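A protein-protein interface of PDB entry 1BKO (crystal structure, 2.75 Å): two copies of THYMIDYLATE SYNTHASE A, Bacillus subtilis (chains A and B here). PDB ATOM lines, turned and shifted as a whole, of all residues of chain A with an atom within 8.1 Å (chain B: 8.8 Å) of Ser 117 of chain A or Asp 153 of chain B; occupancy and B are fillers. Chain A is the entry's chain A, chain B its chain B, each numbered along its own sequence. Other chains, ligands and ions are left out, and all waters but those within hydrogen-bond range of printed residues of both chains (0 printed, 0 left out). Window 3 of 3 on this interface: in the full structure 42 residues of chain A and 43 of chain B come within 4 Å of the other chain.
The side-chain amino group (NZ) of Lys 122 of chain A is in hydrogen-bond range of the backbone carbonyl oxygen (O) of Asn 115 of chain A (2.7 Å). The backbone carbonyl oxygen (O) of Val 123 of chain A sits at hydrogen-bond distance from the backbone NH (N) of Asn 115 of chain A (3.4 Å). N of Val 123 of chain A sits at hydrogen-bond distance from O of Arg 116 of chain A (2.6 Å). The side-chain hydroxyl (OH) of Tyr 128 of chain A lies within hydrogen-bond range of the guanidinium group (NH2) of Arg 116 of chain A, at 3.0 Å. The side-chain amino group of Lys 122 of chain A sits at hydrogen-bond distance from the side-chain hydroxyl of Ser 117 of chain A, at 3.3 Å. The backbone NH (N) of Asp 150 of chain B sits at hydrogen-bond distance from the side-chain amide oxygen (OD1) of Asn 148 of chain B (2.9 Å).
No position is printed for both chains. Of the 7 pairs that touch across the chains among the printed residues, none has its exchanged pair printed and touching as well.
Of the printed residues of chain B, Arg 116 of chain A touches Leu 152 (3.3 Å) and Asp 153 (3.2 Å). Of chain B, only Asp 153 (2.9 Å) comes within 4 Å of Ser 117 of chain A. Of the printed residues of chain A, Pro 149 of chain B touches Asn 115. Of the printed residues of chain A, Asp 153 of chain B touches Asn 115, Arg 116, Ser 117 and Lys 122. The nearest residue of chain B that does not touch Ser 117 of chain A is Leu 152 of chain B (7.9 Å). The nearest printed residue of chain A that does not touch Asp 153 of chain B is Leu 118 of chain A (6.1 Å).
CB of Asn 115 of chain A touches OD1 of Asp 150 of chain B (3.5 Å). O of Asn 115 of chain A touches OD2 of Asp 153 of chain B (3.98 Å). NH1 of Arg 116 of chain A touches CD1 of Leu 152 of chain B, 3.3 Å away.
Of the 15 printed residues of chain B, 4 touch a printed residue of chain A. Printed residues of chain B that touch a printed residue of chain A: Pro 149, Asp 150, Leu 152 and Asp 153. Hydrophobic or aromatic side chains of chain B within 4 Å of the printed part of chain A: Leu 152. Along chain B the printed residues that touch a printed residue of chain A span positions 149 to 153. Among the printed residues, Asp or Glu carboxylates within 4 Å of a Lys or Arg side-chain nitrogen of the other chain: Arg 116 of chain A with Asp 153 of chain B and Lys 122 of chain A with Asp 153 of chain B.
The side-chain amide oxygen of Asn 115 of chain A sits close to the backbone carbonyl oxygen of Pro 149 of chain B, 3.0 Å away. The guanidinium group (NE) of Arg 116 of chain A is in salt-bridge range of the side-chain carboxylate (OD1) of Asp 153 of chain B (3.2 Å). OD2 of Asp 153 of chain B sits at hydrogen-bond distance from OG of Ser 117 of chain A, 2.9 Å away. The side-chain carboxylate of Asp 153 of chain B lies within salt-bridge range of the side-chain amino group of Lys 122 of chain A (3.9 Å).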
ATOM      1  N   LYS A 114     -23.332   1.885  18.624  1.00  0.00           N
ATOM      2  CA  LYS A 114     -23.038   2.845  19.677  1.00  0.00           C
ATOM      3  C   LYS A 114     -22.338   2.123  20.825  1.00  0.00           C
ATOM      4  O   LYS A 114     -22.947   1.816  21.851  1.00  0.00           O
ATOM      5  CB  LYS A 114     -24.328   3.515  20.149  1.00  0.00           C
ATOM      6  CG  LYS A 114     -25.029   4.325  19.062  1.00  0.00           C
ATOM      7  CD  LYS A 114     -26.042   5.292  19.662  1.00  0.00           C
ATOM      8  CE  LYS A 114     -26.436   6.384  18.679  1.00  0.00           C
ATOM      9  NZ  LYS A 114     -27.095   7.521  19.381  1.00  0.00           N
ATOM     10  N   ASN A 115     -21.062   1.818  20.621  1.00  0.00           N
ATOM     11  CA  ASN A 115     -20.282   1.096  21.612  1.00  0.00           C
ATOM     12  C   ASN A 115     -19.327   1.924  22.462  1.00  0.00           C
ATOM     13  O   ASN A 115     -18.925   1.476  23.537  1.00  0.00           O
ATOM     14  CB  ASN A 115     -19.529  -0.061  20.953  1.00  0.00           C
ATOM     15  CG  ASN A 115     -18.642   0.394  19.819  1.00  0.00           C
ATOM     16  OD1 ASN A 115     -17.710   1.170  20.018  1.00  0.00           O
ATOM     17  ND2 ASN A 115     -18.915  -0.104  18.619  1.00  0.00           N
ATOM     18  N   ARG A 116     -18.930   3.098  21.985  1.00  0.00           N
ATOM     19  CA  ARG A 116     -18.021   3.938  22.758  1.00  0.00           C
ATOM     20  C   ARG A 116     -18.745   5.008  23.572  1.00  0.00           C
ATOM     21  O   ARG A 116     -19.870   5.406  23.246  1.00  0.00           O
ATOM     22  CB  ARG A 116     -16.960   4.593  21.864  1.00  0.00           C
ATOM     23  CG  ARG A 116     -15.898   3.640  21.344  1.00  0.00           C
ATOM     24  CD  ARG A 116     -15.067   3.036  22.473  1.00  0.00           C
ATOM     25  NE  ARG A 116     -14.194   4.009  23.131  1.00  0.00           N
ATOM     26  CZ  ARG A 116     -13.052   4.476  22.620  1.00  0.00           C
ATOM     27  NH1 ARG A 116     -12.631   4.066  21.430  1.00  0.00           N
ATOM     28  NH2 ARG A 116     -12.306   5.324  23.316  1.00  0.00           N
ATOM     29  N   SER A 117     -18.080   5.455  24.637  1.00  0.00           N
ATOM     30  CA  SER A 117     -18.597   6.482  25.533  1.00  0.00           C
ATOM     31  C   SER A 117     -17.732   7.730  25.424  1.00  0.00           C
ATOM     32  O   SER A 117     -16.503   7.642  25.310  1.00  0.00           O
ATOM     33  CB  SER A 117     -18.574   5.995  26.985  1.00  0.00           C
ATOM     34  OG  SER A 117     -19.209   4.737  27.125  1.00  0.00           O
ATOM     35  N   LEU A 118     -18.377   8.889  25.478  1.00  0.00           N
ATOM     36  CA  LEU A 118     -17.691  10.172  25.395  1.00  0.00           C
ATOM     37  C   LEU A 118     -18.560  11.247  26.046  1.00  0.00           C
ATOM     38  O   LEU A 118     -19.630  11.593  25.531  1.00  0.00           O
ATOM     39  CB  LEU A 118     -17.407  10.535  23.934  1.00  0.00           C
ATOM     40  CG  LEU A 118     -16.947  11.967  23.644  1.00  0.00           C
ATOM     41  CD1 LEU A 118     -15.460  11.993  23.333  1.00  0.00           C
ATOM     42  CD2 LEU A 118     -17.747  12.538  22.480  1.00  0.00           C
ATOM     43  N   ASN A 119     -18.095  11.756  27.188  1.00  0.00           N
ATOM     44  CA  ASN A 119     -18.810  12.789  27.934  1.00  0.00           C
ATOM     45  C   ASN A 119     -20.185  12.269  28.358  1.00  0.00           C
ATOM     46  O   ASN A 119     -21.213  12.889  28.063  1.00  0.00           O
ATOM     47  CB  ASN A 119     -18.966  14.065  27.088  1.00  0.00           C
ATOM     48  CG  ASN A 119     -17.633  14.674  26.678  1.00  0.00           C
ATOM     49  OD1 ASN A 119     -17.481  15.168  25.555  1.00  0.00           O
ATOM     50  ND2 ASN A 119     -16.662  14.661  27.593  1.00  0.00           N
ATOM     51  N   GLY A 120     -20.193  11.131  29.053  1.00  0.00           N
ATOM     52  CA  GLY A 120     -21.438  10.530  29.505  1.00  0.00           C
ATOM     53  C   GLY A 120     -22.446  10.305  28.386  1.00  0.00           C
ATOM     54  O   GLY A 120     -23.656  10.468  28.582  1.00  0.00           O
ATOM     55  N   GLU A 121     -21.954   9.887  27.224  1.00  0.00           N
ATOM     56  CA  GLU A 121     -22.812   9.661  26.068  1.00  0.00           C
ATOM     57  C   GLU A 121     -22.352   8.422  25.294  1.00  0.00           C
ATOM     58  O   GLU A 121     -21.177   8.062  25.340  1.00  0.00           O
ATOM     59  CB  GLU A 121     -22.761  10.899  25.159  1.00  0.00           C
ATOM     60  CG  GLU A 121     -23.940  11.049  24.218  1.00  0.00           C
ATOM     61  CD  GLU A 121     -25.260  11.177  24.959  1.00  0.00           C
ATOM     62  OE1 GLU A 121     -25.484  12.218  25.616  1.00  0.00           O
ATOM     63  OE2 GLU A 121     -26.073  10.233  24.885  1.00  0.00           O
ATOM     64  N   LYS A 122     -23.287   7.748  24.628  1.00  0.00           N
ATOM     65  CA  LYS A 122     -22.951   6.566  23.831  1.00  0.00           C
ATOM     66  C   LYS A 122     -22.798   6.922  22.353  1.00  0.00           C
ATOM     67  O   LYS A 122     -23.768   7.272  21.678  1.00  0.00           O
ATOM     68  CB  LYS A 122     -23.989   5.458  24.018  1.00  0.00           C
ATOM     69  CG  LYS A 122     -23.616   4.463  25.105  1.00  0.00           C
ATOM     70  CD  LYS A 122     -22.268   3.802  24.806  1.00  0.00           C
ATOM     71  CE  LYS A 122     -21.898   2.761  25.855  1.00  0.00           C
ATOM     72  NZ  LYS A 122     -20.580   2.119  25.569  1.00  0.00           N
ATOM     73  N   VAL A 123     -21.573   6.797  21.855  1.00  0.00           N
ATOM     74  CA  VAL A 123     -21.260   7.146  20.477  1.00  0.00           C
ATOM     75  C   VAL A 123     -20.747   5.990  19.610  1.00  0.00           C
ATOM     76  O   VAL A 123     -20.176   5.020  20.113  1.00  0.00           O
ATOM     77  CB  VAL A 123     -20.232   8.301  20.453  1.00  0.00           C
ATOM     78  CG1 VAL A 123     -18.891   7.849  21.031  1.00  0.00           C
ATOM     79  CG2 VAL A 123     -20.062   8.816  19.063  1.00  0.00           C
ATOM     80  N   ASP A 124     -20.982   6.095  18.305  1.00  0.00           N
ATOM     81  CA  ASP A 124     -20.525   5.077  17.372  1.00  0.00           C
ATOM     82  C   ASP A 124     -19.108   5.370  16.887  1.00  0.00           C
ATOM     83  O   ASP A 124     -18.650   6.520  16.943  1.00  0.00           O
ATOM     84  CB  ASP A 124     -21.505   4.893  16.189  1.00  0.00           C
ATOM     85  CG  ASP A 124     -21.613   6.121  15.261  1.00  0.00           C
ATOM     86  OD1 ASP A 124     -20.648   6.896  15.075  1.00  0.00           O
ATOM     87  OD2 ASP A 124     -22.690   6.273  14.659  1.00  0.00           O
ATOM     88  N   TYR A 128     -17.124   9.384  17.329  1.00  0.00           N
ATOM     89  CA  TYR A 128     -16.042   9.442  18.296  1.00  0.00           C
ATOM     90  C   TYR A 128     -14.763   9.936  17.637  1.00  0.00           C
ATOM     91  O   TYR A 128     -14.083  10.802  18.190  1.00  0.00           O
ATOM     92  CB  TYR A 128     -15.801   8.078  18.951  1.00  0.00           C
ATOM     93  CG  TYR A 128     -14.786   8.122  20.088  1.00  0.00           C
ATOM     94  CD1 TYR A 128     -13.416   8.001  19.833  1.00  0.00           C
ATOM     95  CD2 TYR A 128     -15.192   8.316  21.415  1.00  0.00           C
ATOM     96  CE1 TYR A 128     -12.476   8.071  20.866  1.00  0.00           C
ATOM     97  CE2 TYR A 128     -14.259   8.389  22.454  1.00  0.00           C
ATOM     98  CZ  TYR A 128     -12.901   8.265  22.173  1.00  0.00           C
ATOM     99  OH  TYR A 128     -11.964   8.309  23.190  1.00  0.00           O
ATOM    100  N   GLN A 132     -12.410  13.346  18.829  1.00  0.00           N
ATOM    101  CA  GLN A 132     -11.016  13.261  19.247  1.00  0.00           C
ATOM    102  C   GLN A 132     -10.049  13.894  18.258  1.00  0.00           C
ATOM    103  O   GLN A 132      -8.919  14.208  18.617  1.00  0.00           O
ATOM    104  CB  GLN A 132     -10.598  11.805  19.429  1.00  0.00           C
ATOM    105  CG  GLN A 132     -11.459  11.017  20.387  1.00  0.00           C
ATOM    106  CD  GLN A 132     -11.419  11.567  21.792  1.00  0.00           C
ATOM    107  OE1 GLN A 132     -12.423  12.074  22.305  1.00  0.00           O
ATOM    108  NE2 GLN A 132     -10.254  11.484  22.423  1.00  0.00           N
ATOM    109  N   GLN B  98      -6.056  -4.504  38.397  1.00  0.00           N
ATOM    110  CA  GLN B  98      -7.361  -3.929  38.715  1.00  0.00           C
ATOM    111  C   GLN B  98      -7.837  -4.393  40.083  1.00  0.00           C
ATOM    112  O   GLN B  98      -7.076  -4.992  40.847  1.00  0.00           O
ATOM    113  CB  GLN B  98      -8.402  -4.321  37.662  1.00  0.00           C
ATOM    114  CG  GLN B  98      -8.258  -3.605  36.328  1.00  0.00           C
ATOM    115  CD  GLN B  98      -8.528  -2.110  36.412  1.00  0.00           C
ATOM    116  OE1 GLN B  98      -8.329  -1.380  35.438  1.00  0.00           O
ATOM    117  NE2 GLN B  98      -9.003  -1.648  37.570  1.00  0.00           N
ATOM    118  N   ILE B 103      -6.838  -7.179  33.906  1.00  0.00           N
ATOM    119  CA  ILE B 103      -6.674  -6.020  33.034  1.00  0.00           C
ATOM    120  C   ILE B 103      -7.989  -5.920  32.272  1.00  0.00           C
ATOM    121  O   ILE B 103      -8.056  -5.375  31.169  1.00  0.00           O
ATOM    122  CB  ILE B 103      -5.513  -6.197  32.036  1.00  0.00           C
ATOM    123  CG1 ILE B 103      -5.613  -7.565  31.353  1.00  0.00           C
ATOM    124  CG2 ILE B 103      -4.180  -5.996  32.752  1.00  0.00           C
ATOM    125  CD1 ILE B 103      -4.730  -7.720  30.125  1.00  0.00           C
ATOM    126  N   GLY B 104      -9.034  -6.481  32.876  1.00  0.00           N
ATOM    127  CA  GLY B 104     -10.346  -6.474  32.262  1.00  0.00           C
ATOM    128  C   GLY B 104     -10.377  -7.312  31.000  1.00  0.00           C
ATOM    129  O   GLY B 104      -9.543  -8.202  30.795  1.00  0.00           O
ATOM    130  N   HIS B 105     -11.350  -7.011  30.150  1.00  0.00           N
ATOM    131  CA  HIS B 105     -11.544  -7.710  28.890  1.00  0.00           C
ATOM    132  C   HIS B 105     -10.446  -7.377  27.876  1.00  0.00           C
ATOM    133  O   HIS B 105     -10.693  -6.737  26.851  1.00  0.00           O
ATOM    134  CB  HIS B 105     -12.926  -7.355  28.343  1.00  0.00           C
ATOM    135  CG  HIS B 105     -14.040  -7.633  29.305  1.00  0.00           C
ATOM    136  ND1 HIS B 105     -15.232  -6.938  29.290  1.00  0.00           N
ATOM    137  CD2 HIS B 105     -14.143  -8.532  30.312  1.00  0.00           C
ATOM    138  CE1 HIS B 105     -16.020  -7.398  30.244  1.00  0.00           C
ATOM    139  NE2 HIS B 105     -15.383  -8.367  30.879  1.00  0.00           N
ATOM    140  N   ASN B 148     -11.071  -5.315  19.763  1.00  0.00           N
ATOM    141  CA  ASN B 148     -12.522  -5.488  19.706  1.00  0.00           C
ATOM    142  C   ASN B 148     -13.195  -4.121  19.958  1.00  0.00           C
ATOM    143  O   ASN B 148     -13.180  -3.600  21.074  1.00  0.00           O
ATOM    144  CB  ASN B 148     -12.944  -6.514  20.758  1.00  0.00           C
ATOM    145  CG  ASN B 148     -14.430  -6.799  20.742  1.00  0.00           C
ATOM    146  OD1 ASN B 148     -15.228  -6.012  20.235  1.00  0.00           O
ATOM    147  ND2 ASN B 148     -14.814  -7.931  21.321  1.00  0.00           N
ATOM    148  N   PRO B 149     -13.812  -3.534  18.918  1.00  0.00           N
ATOM    149  CA  PRO B 149     -14.474  -2.225  19.053  1.00  0.00           C
ATOM    150  C   PRO B 149     -15.582  -2.169  20.114  1.00  0.00           C
ATOM    151  O   PRO B 149     -15.886  -1.099  20.646  1.00  0.00           O
ATOM    152  CB  PRO B 149     -15.021  -1.964  17.645  1.00  0.00           C
ATOM    153  CG  PRO B 149     -15.310  -3.343  17.131  1.00  0.00           C
ATOM    154  CD  PRO B 149     -14.123  -4.154  17.614  1.00  0.00           C
ATOM    155  N   ASP B 150     -16.185  -3.319  20.404  1.00  0.00           N
ATOM    156  CA  ASP B 150     -17.256  -3.395  21.389  1.00  0.00           C
ATOM    157  C   ASP B 150     -16.761  -3.459  22.827  1.00  0.00           C
ATOM    158  O   ASP B 150     -17.561  -3.341  23.757  1.00  0.00           O
ATOM    159  CB  ASP B 150     -18.159  -4.611  21.119  1.00  0.00           C
ATOM    160  CG  ASP B 150     -19.167  -4.363  20.007  1.00  0.00           C
ATOM    161  OD1 ASP B 150     -20.015  -3.453  20.162  1.00  0.00           O
ATOM    162  OD2 ASP B 150     -19.127  -5.089  18.986  1.00  0.00           O
ATOM    163  N   GLU B 151     -15.461  -3.648  23.024  1.00  0.00           N
ATOM    164  CA  GLU B 151     -14.929  -3.758  24.381  1.00  0.00           C
ATOM    165  C   GLU B 151     -13.721  -2.893  24.748  1.00  0.00           C
ATOM    166  O   GLU B 151     -12.990  -3.210  25.691  1.00  0.00           O
ATOM    167  CB  GLU B 151     -14.654  -5.230  24.718  1.00  0.00           C
ATOM    168  CG  GLU B 151     -15.912  -6.078  24.789  1.00  0.00           C
ATOM    169  CD  GLU B 151     -15.644  -7.487  25.247  1.00  0.00           C
ATOM    170  OE1 GLU B 151     -15.324  -7.670  26.434  1.00  0.00           O
ATOM    171  OE2 GLU B 151     -15.758  -8.420  24.423  1.00  0.00           O
ATOM    172  N   LEU B 152     -13.533  -1.785  24.036  1.00  0.00           N
ATOM    173  CA  LEU B 152     -12.423  -0.875  24.325  1.00  0.00           C
ATOM    174  C   LEU B 152     -12.603  -0.212  25.700  1.00  0.00           C
ATOM    175  O   LEU B 152     -11.625   0.054  26.408  1.00  0.00           O
ATOM    176  CB  LEU B 152     -12.330   0.207  23.245  1.00  0.00           C
ATOM    177  CG  LEU B 152     -12.059  -0.254  21.813  1.00  0.00           C
ATOM    178  CD1 LEU B 152     -12.434   0.856  20.843  1.00  0.00           C
ATOM    179  CD2 LEU B 152     -10.606  -0.666  21.652  1.00  0.00           C
ATOM    180  N   ASP B 153     -13.857   0.075  26.051  1.00  0.00           N
ATOM    181  CA  ASP B 153     -14.193   0.705  27.330  1.00  0.00           C
ATOM    182  C   ASP B 153     -13.969  -0.188  28.551  1.00  0.00           C
ATOM    183  O   ASP B 153     -13.637   0.306  29.625  1.00  0.00           O
ATOM    184  CB  ASP B 153     -15.644   1.212  27.318  1.00  0.00           C
ATOM    185  CG  ASP B 153     -15.803   2.578  26.631  1.00  0.00           C
ATOM    186  OD1 ASP B 153     -14.808   3.163  26.135  1.00  0.00           O
ATOM    187  OD2 ASP B 153     -16.947   3.077  26.599  1.00  0.00           O
ATOM    188  N   ALA B 154     -14.176  -1.492  28.396  1.00  0.00           N
ATOM    189  CA  ALA B 154     -14.000  -2.424  29.507  1.00  0.00           C
ATOM    190  C   ALA B 154     -12.596  -3.023  29.587  1.00  0.00           C
ATOM    191  O   ALA B 154     -12.421  -4.157  30.050  1.00  0.00           O
ATOM    192  CB  ALA B 154     -15.058  -3.529  29.445  1.00  0.00           C
ATOM    193  N   MET B 155     -11.601  -2.257  29.150  1.00  0.00           N
ATOM    194  CA  MET B 155     -10.210  -2.706  29.177  1.00  0.00           C
ATOM    195  C   MET B 155      -9.358  -1.813  30.064  1.00  0.00           C
ATOM    196  O   MET B 155      -9.569  -0.600  30.105  1.00  0.00           O
ATOM    197  CB  MET B 155      -9.628  -2.728  27.762  1.00  0.00           C
ATOM    198  CG  MET B 155     -10.043  -3.957  26.978  1.00  0.00           C
ATOM    199  SD  MET B 155      -9.872  -3.866  25.183  1.00  0.00           S
ATOM    200  CE  MET B 155      -8.134  -4.197  24.979  1.00  0.00           C
ATOM    201  N   ALA B 156      -8.428  -2.406  30.809  1.00  0.00           N
ATOM    202  CA  ALA B 156      -7.546  -1.617  31.670  1.00  0.00           C
ATOM    203  C   ALA B 156      -6.648  -0.793  30.754  1.00  0.00           C
ATOM    204  O   ALA B 156      -6.121   0.257  31.145  1.00  0.00           O
ATOM    205  CB  ALA B 156      -6.702  -2.515  32.570  1.00  0.00           C
ATOM    206  N   LEU B 157      -6.463  -1.291  29.535  1.00  0.00           N
ATOM    207  CA  LEU B 157      -5.641  -0.596  28.563  1.00  0.00           C
ATOM    208  C   LEU B 157      -5.788  -1.118  27.138  1.00  0.00           C
ATOM    209  O   LEU B 157      -6.268  -2.232  26.904  1.00  0.00           O
ATOM    210  CB  LEU B 157      -4.160  -0.595  28.987  1.00  0.00           C
ATOM    211  CG  LEU B 157      -3.350  -1.891  29.110  1.00  0.00           C
ATOM    212  CD1 LEU B 157      -1.908  -1.540  29.446  1.00  0.00           C
ATOM    213  CD2 LEU B 157      -3.932  -2.803  30.182  1.00  0.00           C
ATOM    214  N   THR B 158      -5.421  -0.268  26.186  1.00  0.00           N
ATOM    215  CA  THR B 158      -5.481  -0.623  24.790  1.00  0.00           C
ATOM    216  C   THR B 158      -4.123  -1.188  24.399  1.00  0.00           C
ATOM    217  O   THR B 158      -3.082  -0.625  24.748  1.00  0.00           O
ATOM    218  CB  THR B 158      -5.872   0.591  23.924  1.00  0.00           C
ATOM    219  OG1 THR B 158      -5.125   1.746  24.328  1.00  0.00           O
ATOM    220  CG2 THR B 158      -7.359   0.876  24.077  1.00  0.00           C
